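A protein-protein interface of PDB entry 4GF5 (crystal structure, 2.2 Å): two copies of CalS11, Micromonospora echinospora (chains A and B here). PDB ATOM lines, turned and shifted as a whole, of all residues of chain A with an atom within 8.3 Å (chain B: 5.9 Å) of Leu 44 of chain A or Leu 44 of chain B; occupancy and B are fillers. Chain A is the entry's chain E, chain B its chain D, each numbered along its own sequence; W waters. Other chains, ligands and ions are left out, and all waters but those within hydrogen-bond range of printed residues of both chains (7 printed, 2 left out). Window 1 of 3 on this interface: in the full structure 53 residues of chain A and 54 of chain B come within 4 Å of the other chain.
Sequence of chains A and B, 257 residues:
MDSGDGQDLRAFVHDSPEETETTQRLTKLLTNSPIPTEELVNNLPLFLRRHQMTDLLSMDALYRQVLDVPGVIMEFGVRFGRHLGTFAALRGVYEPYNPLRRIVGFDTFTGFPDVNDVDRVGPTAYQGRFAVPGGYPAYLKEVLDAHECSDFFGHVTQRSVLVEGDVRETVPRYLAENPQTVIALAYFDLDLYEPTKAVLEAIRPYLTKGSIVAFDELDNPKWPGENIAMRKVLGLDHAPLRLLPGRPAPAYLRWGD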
ATOM      1  N   LEU A  26      -9.136  10.843  12.872  1.00  0.00           N
ATOM      2  CA  LEU A  26      -8.005  11.767  12.950  1.00  0.00           C
ATOM      3  C   LEU A  26      -7.092  11.369  14.096  1.00  0.00           C
ATOM      4  O   LEU A  26      -5.873  11.496  13.990  1.00  0.00           O
ATOM      5  CB  LEU A  26      -8.462  13.227  13.118  1.00  0.00           C
ATOM      6  CG  LEU A  26      -9.097  13.895  11.895  1.00  0.00           C
ATOM      7  CD1 LEU A  26      -9.608  15.293  12.239  1.00  0.00           C
ATOM      8  CD2 LEU A  26      -8.130  13.949  10.693  1.00  0.00           C
ATOM      9  N   THR A  27      -7.689  10.907  15.193  1.00  0.00           N
ATOM     10  CA  THR A  27      -6.922  10.302  16.274  1.00  0.00           C
ATOM     11  C   THR A  27      -6.057   9.150  15.746  1.00  0.00           C
ATOM     12  O   THR A  27      -4.849   9.113  15.992  1.00  0.00           O
ATOM     13  CB  THR A  27      -7.820   9.796  17.420  1.00  0.00           C
ATOM     14  OG1 THR A  27      -8.434  10.916  18.071  1.00  0.00           O
ATOM     15  CG2 THR A  27      -7.000   9.022  18.446  1.00  0.00           C
ATOM     16  N   LEU A  30      -3.269  10.375  13.561  1.00  0.00           N
ATOM     17  CA  LEU A  30      -2.265  11.119  14.303  1.00  0.00           C
ATOM     18  C   LEU A  30      -1.243  10.162  14.918  1.00  0.00           C
ATOM     19  O   LEU A  30      -0.034  10.346  14.779  1.00  0.00           O
ATOM     20  CB  LEU A  30      -2.933  11.943  15.406  1.00  0.00           C
ATOM     21  CG  LEU A  30      -1.982  12.694  16.338  1.00  0.00           C
ATOM     22  CD1 LEU A  30      -1.079  13.624  15.537  1.00  0.00           C
ATOM     23  CD2 LEU A  30      -2.764  13.457  17.410  1.00  0.00           C
ATOM     24  N   ILE A  35       4.445  10.718   8.888  1.00  0.00           N
ATOM     25  CA  ILE A  35       5.217  11.946   9.064  1.00  0.00           C
ATOM     26  C   ILE A  35       6.310  11.652  10.075  1.00  0.00           C
ATOM     27  O   ILE A  35       6.033  11.040  11.097  1.00  0.00           O
ATOM     28  CB  ILE A  35       4.315  13.084   9.584  1.00  0.00           C
ATOM     29  CG1 ILE A  35       3.245  13.426   8.541  1.00  0.00           C
ATOM     30  CG2 ILE A  35       5.119  14.318   9.939  1.00  0.00           C
ATOM     31  CD1 ILE A  35       2.100  14.260   9.100  1.00  0.00           C
ATOM     32  N   GLU A  39       8.419  16.085  12.918  1.00  0.00           N
ATOM     33  CA  GLU A  39       7.739  17.052  12.056  1.00  0.00           C
ATOM     34  C   GLU A  39       6.276  17.186  12.439  1.00  0.00           C
ATOM     35  O   GLU A  39       5.569  18.057  11.924  1.00  0.00           O
ATOM     36  CB  GLU A  39       7.846  16.656  10.581  1.00  0.00           C
ATOM     37  CG  GLU A  39       9.208  16.932   9.955  1.00  0.00           C
ATOM     38  CD  GLU A  39       9.578  18.402   9.943  1.00  0.00           C
ATOM     39  OE1 GLU A  39       8.670  19.264   9.907  1.00  0.00           O
ATOM     40  OE2 GLU A  39      10.786  18.703   9.963  1.00  0.00           O
ATOM     41  N   LEU A  40       5.837  16.321  13.349  1.00  0.00           N
ATOM     42  CA  LEU A  40       4.439  16.247  13.742  1.00  0.00           C
ATOM     43  C   LEU A  40       3.929  17.572  14.294  1.00  0.00           C
ATOM     44  O   LEU A  40       2.845  18.014  13.919  1.00  0.00           O
ATOM     45  CB  LEU A  40       4.212  15.122  14.757  1.00  0.00           C
ATOM     46  CG  LEU A  40       3.625  13.831  14.180  1.00  0.00           C
ATOM     47  CD1 LEU A  40       3.391  12.793  15.270  1.00  0.00           C
ATOM     48  CD2 LEU A  40       2.339  14.145  13.453  1.00  0.00           C
ATOM     49  N   VAL A  41       4.714  18.208  15.163  1.00  0.00           N
ATOM     50  CA  VAL A  41       4.306  19.483  15.748  1.00  0.00           C
ATOM     51  C   VAL A  41       4.350  20.614  14.720  1.00  0.00           C
ATOM     52  O   VAL A  41       3.974  21.751  15.031  1.00  0.00           O
ATOM     53  CB  VAL A  41       5.157  19.881  16.997  1.00  0.00           C
ATOM     54  CG1 VAL A  41       4.943  18.900  18.123  1.00  0.00           C
ATOM     55  CG2 VAL A  41       6.627  20.003  16.651  1.00  0.00           C
ATOM     56  N   ASN A  42       4.826  20.305  13.516  1.00  0.00           N
ATOM     57  CA  ASN A  42       4.810  21.268  12.416  1.00  0.00           C
ATOM     58  C   ASN A  42       3.637  21.025  11.467  1.00  0.00           C
ATOM     59  O   ASN A  42       3.523  21.679  10.425  1.00  0.00           O
ATOM     60  CB  ASN A  42       6.113  21.213  11.621  1.00  0.00           C
ATOM     61  CG  ASN A  42       7.298  21.673  12.423  1.00  0.00           C
ATOM     62  OD1 ASN A  42       7.148  22.418  13.396  1.00  0.00           O
ATOM     63  ND2 ASN A  42       8.494  21.223  12.035  1.00  0.00           N
ATOM     64  N   ASN A  43       2.779  20.076  11.815  1.00  0.00           N
ATOM     65  CA  ASN A  43       1.675  19.702  10.933  1.00  0.00           C
ATOM     66  C   ASN A  43       0.381  19.400  11.674  1.00  0.00           C
ATOM     67  O   ASN A  43      -0.518  18.747  11.131  1.00  0.00           O
ATOM     68  CB  ASN A  43       2.065  18.517  10.042  1.00  0.00           C
ATOM     69  CG  ASN A  43       3.202  18.857   9.099  1.00  0.00           C
ATOM     70  OD1 ASN A  43       2.988  19.432   8.024  1.00  0.00           O
ATOM     71  ND2 ASN A  43       4.425  18.515   9.499  1.00  0.00           N
ATOM     72  N   LEU A  44       0.282  19.893  12.907  1.00  0.00           N
ATOM     73  CA  LEU A  44      -0.906  19.673  13.725  1.00  0.00           C
ATOM     74  C   LEU A  44      -2.253  20.035  13.066  1.00  0.00           C
ATOM     75  O   LEU A  44      -3.249  19.383  13.361  1.00  0.00           O
ATOM     76  CB  LEU A  44      -0.764  20.349  15.101  1.00  0.00           C
ATOM     77  CG  LEU A  44       0.391  19.853  15.984  1.00  0.00           C
ATOM     78  CD1 LEU A  44       0.480  20.650  17.283  1.00  0.00           C
ATOM     79  CD2 LEU A  44       0.260  18.362  16.293  1.00  0.00           C
ATOM     80  N   PRO A  45      -2.301  21.064  12.186  1.00  0.00           N
ATOM     81  CA  PRO A  45      -3.617  21.366  11.593  1.00  0.00           C
ATOM     82  C   PRO A  45      -4.253  20.218  10.812  1.00  0.00           C
ATOM     83  O   PRO A  45      -5.479  20.189  10.678  1.00  0.00           O
ATOM     84  CB  PRO A  45      -3.317  22.543  10.669  1.00  0.00           C
ATOM     85  CG  PRO A  45      -2.243  23.287  11.395  1.00  0.00           C
ATOM     86  CD  PRO A  45      -1.369  22.194  11.998  1.00  0.00           C
ATOM     87  N   LEU A  46      -3.445  19.274  10.338  1.00  0.00           N
ATOM     88  CA  LEU A  46      -3.976  18.077   9.696  1.00  0.00           C
ATOM     89  C   LEU A  46      -5.037  17.421  10.558  1.00  0.00           C
ATOM     90  O   LEU A  46      -6.011  16.870  10.045  1.00  0.00           O
ATOM     91  CB  LEU A  46      -2.854  17.063   9.438  1.00  0.00           C
ATOM     92  CG  LEU A  46      -1.872  17.445   8.333  1.00  0.00           C
ATOM     93  CD1 LEU A  46      -0.745  16.427   8.254  1.00  0.00           C
ATOM     94  CD2 LEU A  46      -2.594  17.582   7.000  1.00  0.00           C
ATOM     95  N   PHE A  47      -4.842  17.488  11.872  1.00  0.00           N
ATOM     96  CA  PHE A  47      -5.653  16.734  12.804  1.00  0.00           C
ATOM     97  C   PHE A  47      -6.578  17.635  13.600  1.00  0.00           C
ATOM     98  O   PHE A  47      -7.282  17.181  14.504  1.00  0.00           O
ATOM     99  CB  PHE A  47      -4.730  15.937  13.716  1.00  0.00           C
ATOM    100  CG  PHE A  47      -3.649  15.240  12.967  1.00  0.00           C
ATOM    101  CD1 PHE A  47      -3.929  14.085  12.256  1.00  0.00           C
ATOM    102  CD2 PHE A  47      -2.367  15.772  12.913  1.00  0.00           C
ATOM    103  CE1 PHE A  47      -2.933  13.438  11.526  1.00  0.00           C
ATOM    104  CE2 PHE A  47      -1.358  15.138  12.188  1.00  0.00           C
ATOM    105  CZ  PHE A  47      -1.648  13.962  11.489  1.00  0.00           C
ATOM    106  N   LEU A  48      -6.594  18.911  13.236  1.00  0.00           N
ATOM    107  CA  LEU A  48      -7.438  19.885  13.931  1.00  0.00           C
ATOM    108  C   LEU A  48      -8.755  20.085  13.183  1.00  0.00           C
ATOM    109  O   LEU A  48      -8.818  20.866  12.232  1.00  0.00           O
ATOM    110  CB  LEU A  48      -6.709  21.227  14.082  1.00  0.00           C
ATOM    111  CG  LEU A  48      -7.390  22.288  14.951  1.00  0.00           C
ATOM    112  CD1 LEU A  48      -7.230  21.948  16.419  1.00  0.00           C
ATOM    113  CD2 LEU A  48      -6.817  23.676  14.648  1.00  0.00           C
ATOM    114  N   ARG A  49      -9.797  19.381  13.621  1.00  0.00           N
ATOM    115  CA  ARG A  49     -11.099  19.441  12.953  1.00  0.00           C
ATOM    116  C   ARG A  49     -11.859  20.760  13.185  1.00  0.00           C
ATOM    117  O   ARG A  49     -11.568  21.482  14.135  1.00  0.00           O
ATOM    118  CB  ARG A  49     -11.962  18.261  13.394  1.00  0.00           C
ATOM    119  CG  ARG A  49     -12.519  18.371  14.810  1.00  0.00           C
ATOM    120  CD  ARG A  49     -13.201  17.066  15.205  1.00  0.00           C
ATOM    121  NE  ARG A  49     -13.828  17.136  16.518  1.00  0.00           N
ATOM    122  CZ  ARG A  49     -13.182  16.975  17.671  1.00  0.00           C
ATOM    123  NH1 ARG A  49     -11.870  16.751  17.676  1.00  0.00           N
ATOM    124  NH2 ARG A  49     -13.846  17.051  18.823  1.00  0.00           N
ATOM    125  N   GLN A  52     -12.754  22.046  16.670  1.00  0.00           N
ATOM    126  CA  GLN A  52     -11.622  22.513  17.481  1.00  0.00           C
ATOM    127  C   GLN A  52     -10.973  23.768  16.903  1.00  0.00           C
ATOM    128  O   GLN A  52     -10.517  24.648  17.646  1.00  0.00           O
ATOM    129  CB  GLN A  52     -10.564  21.414  17.664  1.00  0.00           C
ATOM    130  CG  GLN A  52     -11.062  20.178  18.399  1.00  0.00           C
ATOM    131  CD  GLN A  52     -11.670  20.504  19.761  1.00  0.00           C
ATOM    132  OE1 GLN A  52     -11.283  21.470  20.422  1.00  0.00           O
ATOM    133  NE2 GLN A  52     -12.632  19.697  20.180  1.00  0.00           N
ATOM    134  N   MET A  53     -10.920  23.838  15.579  1.00  0.00           N
ATOM    135  CA  MET A  53     -10.438  25.034  14.907  1.00  0.00           C
ATOM    136  C   MET A  53     -11.310  26.221  15.315  1.00  0.00           C
ATOM    137  O   MET A  53     -10.804  27.308  15.574  1.00  0.00           O
ATOM    138  CB  MET A  53     -10.481  24.851  13.388  1.00  0.00           C
ATOM    139  CG  MET A  53     -10.232  26.134  12.600  1.00  0.00           C
ATOM    140  SD  MET A  53      -8.512  26.686  12.710  1.00  0.00           S
ATOM    141  CE  MET A  53      -7.749  25.747  11.395  1.00  0.00           C
ATOM    142  N   LEU A  56     -10.391  27.576  18.620  1.00  0.00           N
ATOM    143  CA  LEU A  56      -9.133  28.281  18.542  1.00  0.00           C
ATOM    144  C   LEU A  56      -9.381  29.683  17.986  1.00  0.00           C
ATOM    145  O   LEU A  56      -8.793  30.657  18.451  1.00  0.00           O
ATOM    146  CB  LEU A  56      -8.163  27.502  17.650  1.00  0.00           C
ATOM    147  CG  LEU A  56      -6.711  27.979  17.562  1.00  0.00           C
ATOM    148  CD1 LEU A  56      -5.839  26.860  17.013  1.00  0.00           C
ATOM    149  CD2 LEU A  56      -6.591  29.190  16.675  1.00  0.00           C
ATOM    150  N   GLY A  81      -6.008  21.787  29.585  1.00  0.00           N
ATOM    151  CA  GLY A  81      -5.312  23.022  29.271  1.00  0.00           C
ATOM    152  C   GLY A  81      -5.372  23.488  27.824  1.00  0.00           C
ATOM    153  O   GLY A  81      -4.581  24.342  27.428  1.00  0.00           O
ATOM    154  N   ARG A  82      -6.298  22.938  27.042  1.00  0.00           N
ATOM    155  CA  ARG A  82      -6.517  23.383  25.654  1.00  0.00           C
ATOM    156  C   ARG A  82      -6.421  24.901  25.492  1.00  0.00           C
ATOM    157  O   ARG A  82      -5.664  25.398  24.665  1.00  0.00           O
ATOM    158  CB  ARG A  82      -7.872  22.903  25.110  1.00  0.00           C
ATOM    159  CG  ARG A  82      -8.245  23.563  23.781  1.00  0.00           C
ATOM    160  CD  ARG A  82      -9.576  23.069  23.248  1.00  0.00           C
ATOM    161  NE  ARG A  82     -10.664  23.288  24.191  1.00  0.00           N
ATOM    162  CZ  ARG A  82     -11.957  23.190  23.876  1.00  0.00           C
ATOM    163  NH1 ARG A  82     -12.330  22.878  22.641  1.00  0.00           N
ATOM    164  NH2 ARG A  82     -12.881  23.404  24.799  1.00  0.00           N
ATOM    165  N   GLY A  85      -2.781  26.509  26.427  1.00  0.00           N
ATOM    166  CA  GLY A  85      -1.838  26.397  25.331  1.00  0.00           C
ATOM    167  C   GLY A  85      -2.087  27.453  24.260  1.00  0.00           C
ATOM    168  O   GLY A  85      -1.144  28.076  23.765  1.00  0.00           O
ATOM    169  N   THR A  86      -3.358  27.641  23.899  1.00  0.00           N
ATOM    170  CA  THR A  86      -3.752  28.613  22.886  1.00  0.00           C
ATOM    171  C   THR A  86      -3.309  30.019  23.306  1.00  0.00           C
ATOM    172  O   THR A  86      -2.619  30.710  22.563  1.00  0.00           O
ATOM    173  CB  THR A  86      -5.286  28.606  22.654  1.00  0.00           C
ATOM    174  OG1 THR A  86      -5.725  27.283  22.334  1.00  0.00           O
ATOM    175  CG2 THR A  86      -5.670  29.537  21.520  1.00  0.00           C
ATOM    176  N   VAL A 143       4.504  21.748  29.643  1.00  0.00           N
ATOM    177  CA  VAL A 143       4.037  22.202  28.334  1.00  0.00           C
ATOM    178  C   VAL A 143       4.146  23.716  28.211  1.00  0.00           C
ATOM    179  O   VAL A 143       4.673  24.218  27.222  1.00  0.00           O
ATOM    180  CB  VAL A 143       2.600  21.728  28.016  1.00  0.00           C
ATOM    181  CG1 VAL A 143       2.039  22.455  26.773  1.00  0.00           C
ATOM    182  CG2 VAL A 143       2.582  20.210  27.814  1.00  0.00           C
ATOM    183  N   HIS A 147       6.688  26.391  25.756  1.00  0.00           N
ATOM    184  CA  HIS A 147       6.342  27.546  24.932  1.00  0.00           C
ATOM    185  C   HIS A 147       7.154  28.773  25.362  1.00  0.00           C
ATOM    186  O   HIS A 147       7.717  29.491  24.537  1.00  0.00           O
ATOM    187  CB  HIS A 147       4.855  27.886  25.081  1.00  0.00           C
ATOM    188  CG  HIS A 147       3.929  26.950  24.369  1.00  0.00           C
ATOM    189  ND1 HIS A 147       3.477  27.184  23.085  1.00  0.00           N
ATOM    190  CD2 HIS A 147       3.337  25.803  24.776  1.00  0.00           C
ATOM    191  CE1 HIS A 147       2.662  26.209  22.727  1.00  0.00           C
ATOM    192  NE2 HIS A 147       2.559  25.359  23.735  1.00  0.00           N
ATOM    193  N   LEU B  30       4.210  15.742  23.434  1.00  0.00           N
ATOM    194  CA  LEU B  30       3.085  15.230  22.658  1.00  0.00           C
ATOM    195  C   LEU B  30       3.092  13.705  22.673  1.00  0.00           C
ATOM    196  O   LEU B  30       2.059  13.074  22.885  1.00  0.00           O
ATOM    197  CB  LEU B  30       3.128  15.735  21.207  1.00  0.00           C
ATOM    198  CG  LEU B  30       2.102  15.106  20.263  1.00  0.00           C
ATOM    199  CD1 LEU B  30       0.686  15.241  20.807  1.00  0.00           C
ATOM    200  CD2 LEU B  30       2.191  15.709  18.864  1.00  0.00           C
ATOM    201  N   GLU B  39      -8.227  12.043  23.552  1.00  0.00           N
ATOM    202  CA  GLU B  39      -8.449  13.471  23.782  1.00  0.00           C
ATOM    203  C   GLU B  39      -7.338  14.331  23.206  1.00  0.00           C
ATOM    204  O   GLU B  39      -7.364  15.549  23.343  1.00  0.00           O
ATOM    205  CB  GLU B  39      -8.593  13.756  25.273  1.00  0.00           C
ATOM    206  CG  GLU B  39      -9.800  13.085  25.910  1.00  0.00           C
ATOM    207  CD  GLU B  39     -11.093  13.799  25.588  1.00  0.00           C
ATOM    208  OE1 GLU B  39     -11.047  14.867  24.930  1.00  0.00           O
ATOM    209  OE2 GLU B  39     -12.157  13.296  26.003  1.00  0.00           O
ATOM    210  N   LEU B  40      -6.353  13.696  22.579  1.00  0.00           N
ATOM    211  CA  LEU B  40      -5.260  14.429  21.961  1.00  0.00           C
ATOM    212  C   LEU B  40      -5.758  15.398  20.901  1.00  0.00           C
ATOM    213  O   LEU B  40      -5.311  16.543  20.861  1.00  0.00           O
ATOM    214  CB  LEU B  40      -4.237  13.479  21.342  1.00  0.00           C
ATOM    215  CG  LEU B  40      -3.223  12.889  22.301  1.00  0.00           C
ATOM    216  CD1 LEU B  40      -2.375  11.861  21.575  1.00  0.00           C
ATOM    217  CD2 LEU B  40      -2.371  13.998  22.914  1.00  0.00           C
ATOM    218  N   VAL B  41      -6.682  14.955  20.047  1.00  0.00           N
ATOM    219  CA  VAL B  41      -7.157  15.825  18.968  1.00  0.00           C
ATOM    220  C   VAL B  41      -8.129  16.883  19.471  1.00  0.00           C
ATOM    221  O   VAL B  41      -8.640  17.673  18.685  1.00  0.00           O
ATOM    222  CB  VAL B  41      -7.779  15.055  17.788  1.00  0.00           C
ATOM    223  CG1 VAL B  41      -6.750  14.115  17.171  1.00  0.00           C
ATOM    224  CG2 VAL B  41      -9.048  14.311  18.228  1.00  0.00           C
ATOM    225  N   ASN B  42      -8.372  16.879  20.779  1.00  0.00           N
ATOM    226  CA  ASN B  42      -9.160  17.910  21.440  1.00  0.00           C
ATOM    227  C   ASN B  42      -8.287  18.876  22.214  1.00  0.00           C
ATOM    228  O   ASN B  42      -8.793  19.747  22.912  1.00  0.00           O
ATOM    229  CB  ASN B  42     -10.176  17.297  22.395  1.00  0.00           C
ATOM    230  CG  ASN B  42     -11.239  16.480  21.674  1.00  0.00           C
ATOM    231  OD1 ASN B  42     -11.495  16.677  20.483  1.00  0.00           O
ATOM    232  ND2 ASN B  42     -11.867  15.560  22.400  1.00  0.00           N
ATOM    233  N   ASN B  43      -6.972  18.712  22.103  1.00  0.00           N
ATOM    234  CA  ASN B  43      -6.043  19.541  22.857  1.00  0.00           C
ATOM    235  C   ASN B  43      -4.779  19.849  22.094  1.00  0.00           C
ATOM    236  O   ASN B  43      -3.737  20.070  22.696  1.00  0.00           O
ATOM    237  CB  ASN B  43      -5.672  18.876  24.178  1.00  0.00           C
ATOM    238  CG  ASN B  43      -6.824  18.833  25.149  1.00  0.00           C
ATOM    239  OD1 ASN B  43      -7.078  19.812  25.875  1.00  0.00           O
ATOM    240  ND2 ASN B  43      -7.542  17.694  25.176  1.00  0.00           N
ATOM    241  N   LEU B  44      -4.865  19.856  20.771  1.00  0.00           N
ATOM    242  CA  LEU B  44      -3.685  20.141  19.949  1.00  0.00           C
ATOM    243  C   LEU B  44      -3.031  21.500  20.212  1.00  0.00           C
ATOM    244  O   LEU B  44      -1.812  21.611  20.096  1.00  0.00           O
ATOM    245  CB  LEU B  44      -3.975  19.936  18.452  1.00  0.00           C
ATOM    246  CG  LEU B  44      -4.437  18.512  18.131  1.00  0.00           C
ATOM    247  CD1 LEU B  44      -5.203  18.437  16.819  1.00  0.00           C
ATOM    248  CD2 LEU B  44      -3.255  17.551  18.133  1.00  0.00           C
ATOM    249  N   PRO B  45      -3.817  22.531  20.590  1.00  0.00           N
ATOM    250  CA  PRO B  45      -3.096  23.801  20.786  1.00  0.00           C
ATOM    251  C   PRO B  45      -2.049  23.765  21.900  1.00  0.00           C
ATOM    252  O   PRO B  45      -1.158  24.635  21.941  1.00  0.00           O
ATOM    253  CB  PRO B  45      -4.212  24.799  21.114  1.00  0.00           C
ATOM    254  CG  PRO B  45      -5.431  24.237  20.406  1.00  0.00           C
ATOM    255  CD  PRO B  45      -5.283  22.731  20.558  1.00  0.00           C
ATOM    256  N   LEU B  46      -2.128  22.759  22.769  1.00  0.00           N
ATOM    257  CA  LEU B  46      -1.078  22.557  23.766  1.00  0.00           C
ATOM    258  C   LEU B  46       0.280  22.464  23.097  1.00  0.00           C
ATOM    259  O   LEU B  46       1.285  22.896  23.662  1.00  0.00           O
ATOM    260  CB  LEU B  46      -1.321  21.286  24.579  1.00  0.00           C
ATOM    261  CG  LEU B  46      -2.323  21.385  25.726  1.00  0.00           C
ATOM    262  CD1 LEU B  46      -2.477  20.044  26.421  1.00  0.00           C
ATOM    263  CD2 LEU B  46      -1.900  22.455  26.716  1.00  0.00           C
ATOM    264  N   PHE B  47       0.301  21.931  21.879  1.00  0.00           N
ATOM    265  CA  PHE B  47       1.556  21.620  21.213  1.00  0.00           C
ATOM    266  C   PHE B  47       1.860  22.518  20.026  1.00  0.00           C
ATOM    267  O   PHE B  47       2.895  22.358  19.379  1.00  0.00           O
ATOM    268  CB  PHE B  47       1.585  20.131  20.835  1.00  0.00           C
ATOM    269  CG  PHE B  47       1.174  19.237  21.977  1.00  0.00           C
ATOM    270  CD1 PHE B  47       2.017  19.052  23.065  1.00  0.00           C
ATOM    271  CD2 PHE B  47      -0.080  18.641  21.996  1.00  0.00           C
ATOM    272  CE1 PHE B  47       1.632  18.268  24.119  1.00  0.00           C
ATOM    273  CE2 PHE B  47      -0.471  17.854  23.061  1.00  0.00           C
ATOM    274  CZ  PHE B  47       0.387  17.668  24.120  1.00  0.00           C
ATOM    275  N   LEU B  48       0.977  23.485  19.783  1.00  0.00           N
ATOM    276  CA  LEU B  48       1.079  24.386  18.626  1.00  0.00           C
ATOM    277  C   LEU B  48       1.750  25.697  19.045  1.00  0.00           C
ATOM    278  O   LEU B  48       1.104  26.593  19.599  1.00  0.00           O
ATOM    279  CB  LEU B  48      -0.319  24.676  18.058  1.00  0.00           C
ATOM    280  CG  LEU B  48      -0.482  25.485  16.767  1.00  0.00           C
ATOM    281  CD1 LEU B  48       0.041  24.715  15.579  1.00  0.00           C
ATOM    282  CD2 LEU B  48      -1.955  25.815  16.539  1.00  0.00           C
ATOM    283  N   ARG B  82       0.171  20.520   5.720  1.00  0.00           N
ATOM    284  CA  ARG B  82      -0.238  21.419   6.807  1.00  0.00           C
ATOM    285  C   ARG B  82      -1.346  22.413   6.407  1.00  0.00           C
ATOM    286  O   ARG B  82      -2.356  22.554   7.102  1.00  0.00           O
ATOM    287  CB  ARG B  82       0.975  22.194   7.337  1.00  0.00           C
ATOM    288  CG  ARG B  82       0.609  23.342   8.286  1.00  0.00           C
ATOM    289  CD  ARG B  82       1.833  24.138   8.698  1.00  0.00           C
ATOM    290  NE  ARG B  82       2.527  24.696   7.542  1.00  0.00           N
ATOM    291  CZ  ARG B  82       3.546  25.545   7.627  1.00  0.00           C
ATOM    292  NH1 ARG B  82       3.989  25.931   8.816  1.00  0.00           N
ATOM    293  NH2 ARG B  82       4.121  26.014   6.527  1.00  0.00           N
HETATM  294  O   HOH W   1      -9.521  17.746  16.028  1.00  0.00           O
HETATM  295  O   HOH W   2       3.518  20.272   5.775  1.00  0.00           O
HETATM  296  O   HOH W   3      -8.379  21.961  20.599  1.00  0.00           O
HETATM  297  O   HOH W   4       4.922  22.516   7.889  1.00  0.00           O
HETATM  298  O   HOH W   5     -10.773  20.200  25.226  1.00  0.00           O
HETATM  299  O   HOH W   6      -8.617  20.585  28.176  1.00  0.00           O
HETATM  300  O   HOH W   7       4.268  23.612  17.421  1.00  0.00           O
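A ring nitrogen (NE2) of His 147 of chain A is in hydrogen-bond range of the backbone carbonyl oxygen of Leu 46 of chain B, 2.8 Å away. The backbone NH (N) of Arg 82 of chain A lies close to the side-chain amide oxygen (OD1) of Asn 43 of chain B. NE2 of Gln 52 of chain A is in hydrogen-bond range of OD1 of Asn 42 of chain B (3.2 Å). NH1 of Arg 49 of chain A lies within hydrogen-bond range of OD1 of Asn 42 of chain B, at 2.8 Å.
The backbone carbonyl oxygen of Glu 39 of chain B sits at hydrogen-bond distance from the side-chain amide nitrogen of Asn 43 of chain B (2.8 Å). The side-chain amide oxygen (OE1) of Gln 52 of chain A lies within hydrogen-bond range of the guanidinium group (NH1) of Arg 82 of chain A (2.8 Å). ND2 of Asn 42 of chain A is in hydrogen-bond range of OE1 of Glu 39 of chain A (2.9 Å). O of Glu 39 of chain A lies within hydrogen-bond range of ND2 of Asn 43 of chain A, 2.7 Å away.
OG1 of Thr 27 of chain A touches CG2 of Val 41 of chain B, 3.5 Å away. Asn 43 of chain A touches Arg 82 of chain B (OD1 to CB, 3.5 Å). Leu 44 of chain A touches Leu 48 of chain B (CD1 to N, 3.8 Å). CB of Val 41 of chain B touches O of Phe 47 of chain A (3.9 Å). Leu 48 of chain A touches Leu 44 of chain B (N to CD1, 3.9 Å). NH1 of Arg 49 of chain A touches O of Val 41 of chain B, at 3.5 Å. Gly 81 of chain A touches Leu 46 of chain B (O to CD2, 3.4 Å). CG1 of Val 143 of chain A touches O of Leu 46 of chain B, at 3.2 Å.
Of the printed residues of chain B, Asn 43 of chain A touches Arg 82. Of the printed residues of chain B, Leu 44 of chain A touches Leu 44, Phe 47 and Leu 48. Printed residues of chain B within 4 Å of Gly 85 of chain A: Pro 45. Printed residues of chain B within 4 Å of Val 143 of chain A: Leu 46 (3.2 Å). Leu 40 of chain B touches none of the printed residues of chain A. Printed residues of chain A within 4 Å of Asn 42 of chain B: Arg 49, Gln 52 and Arg 82. Of chain A, only Leu 44, Phe 47 and Leu 48 come within 4 Å of Leu 44 of chain B.
Hydrophobic or aromatic side chains of chain B that line the printed part of chain A: Val 41, Leu 44, Pro 45, Leu 46 and Phe 47. Of the 24 printed residues of chain A, 15 touch a printed residue of chain B. Hydrophobic or aromatic side chains of chain A within 4 Å of the printed part of chain B: Leu 44, Pro 45, Val 143 and His 147.
Asn 42 of chain A touches Arg 82 of chain B, and with the chains exchanged Arg 82 of chain A touches Asn 42 of chain B. Pro 45 of chain A touches Arg 82 of chain B, and with the chains exchanged Arg 82 of chain A touches Pro 45 of chain B. Phe 47 of chain A touches Val 41 of chain B, but with the chains exchanged Val 41 of chain A does not touch Phe 47 of chain B (4.1 Å). 12 positions are printed for both chains.
Water W2 bridges OD1 of Asn 43 of chain A (2.5 Å) and N of Arg 82 of chain B (3.4 Å). Water W6 lies within hydrogen-bond range of OD1 of Asn 43 of chain B (2.9 Å), N of Gly 81 of chain A (3.2 Å) and N of Arg 82 of chain A (3.5 Å). Water W3 lies within hydrogen-bond range of OE1 of Gln 52 of chain A (3.0 Å) and O of Asn 42 of chain B (3.2 Å).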
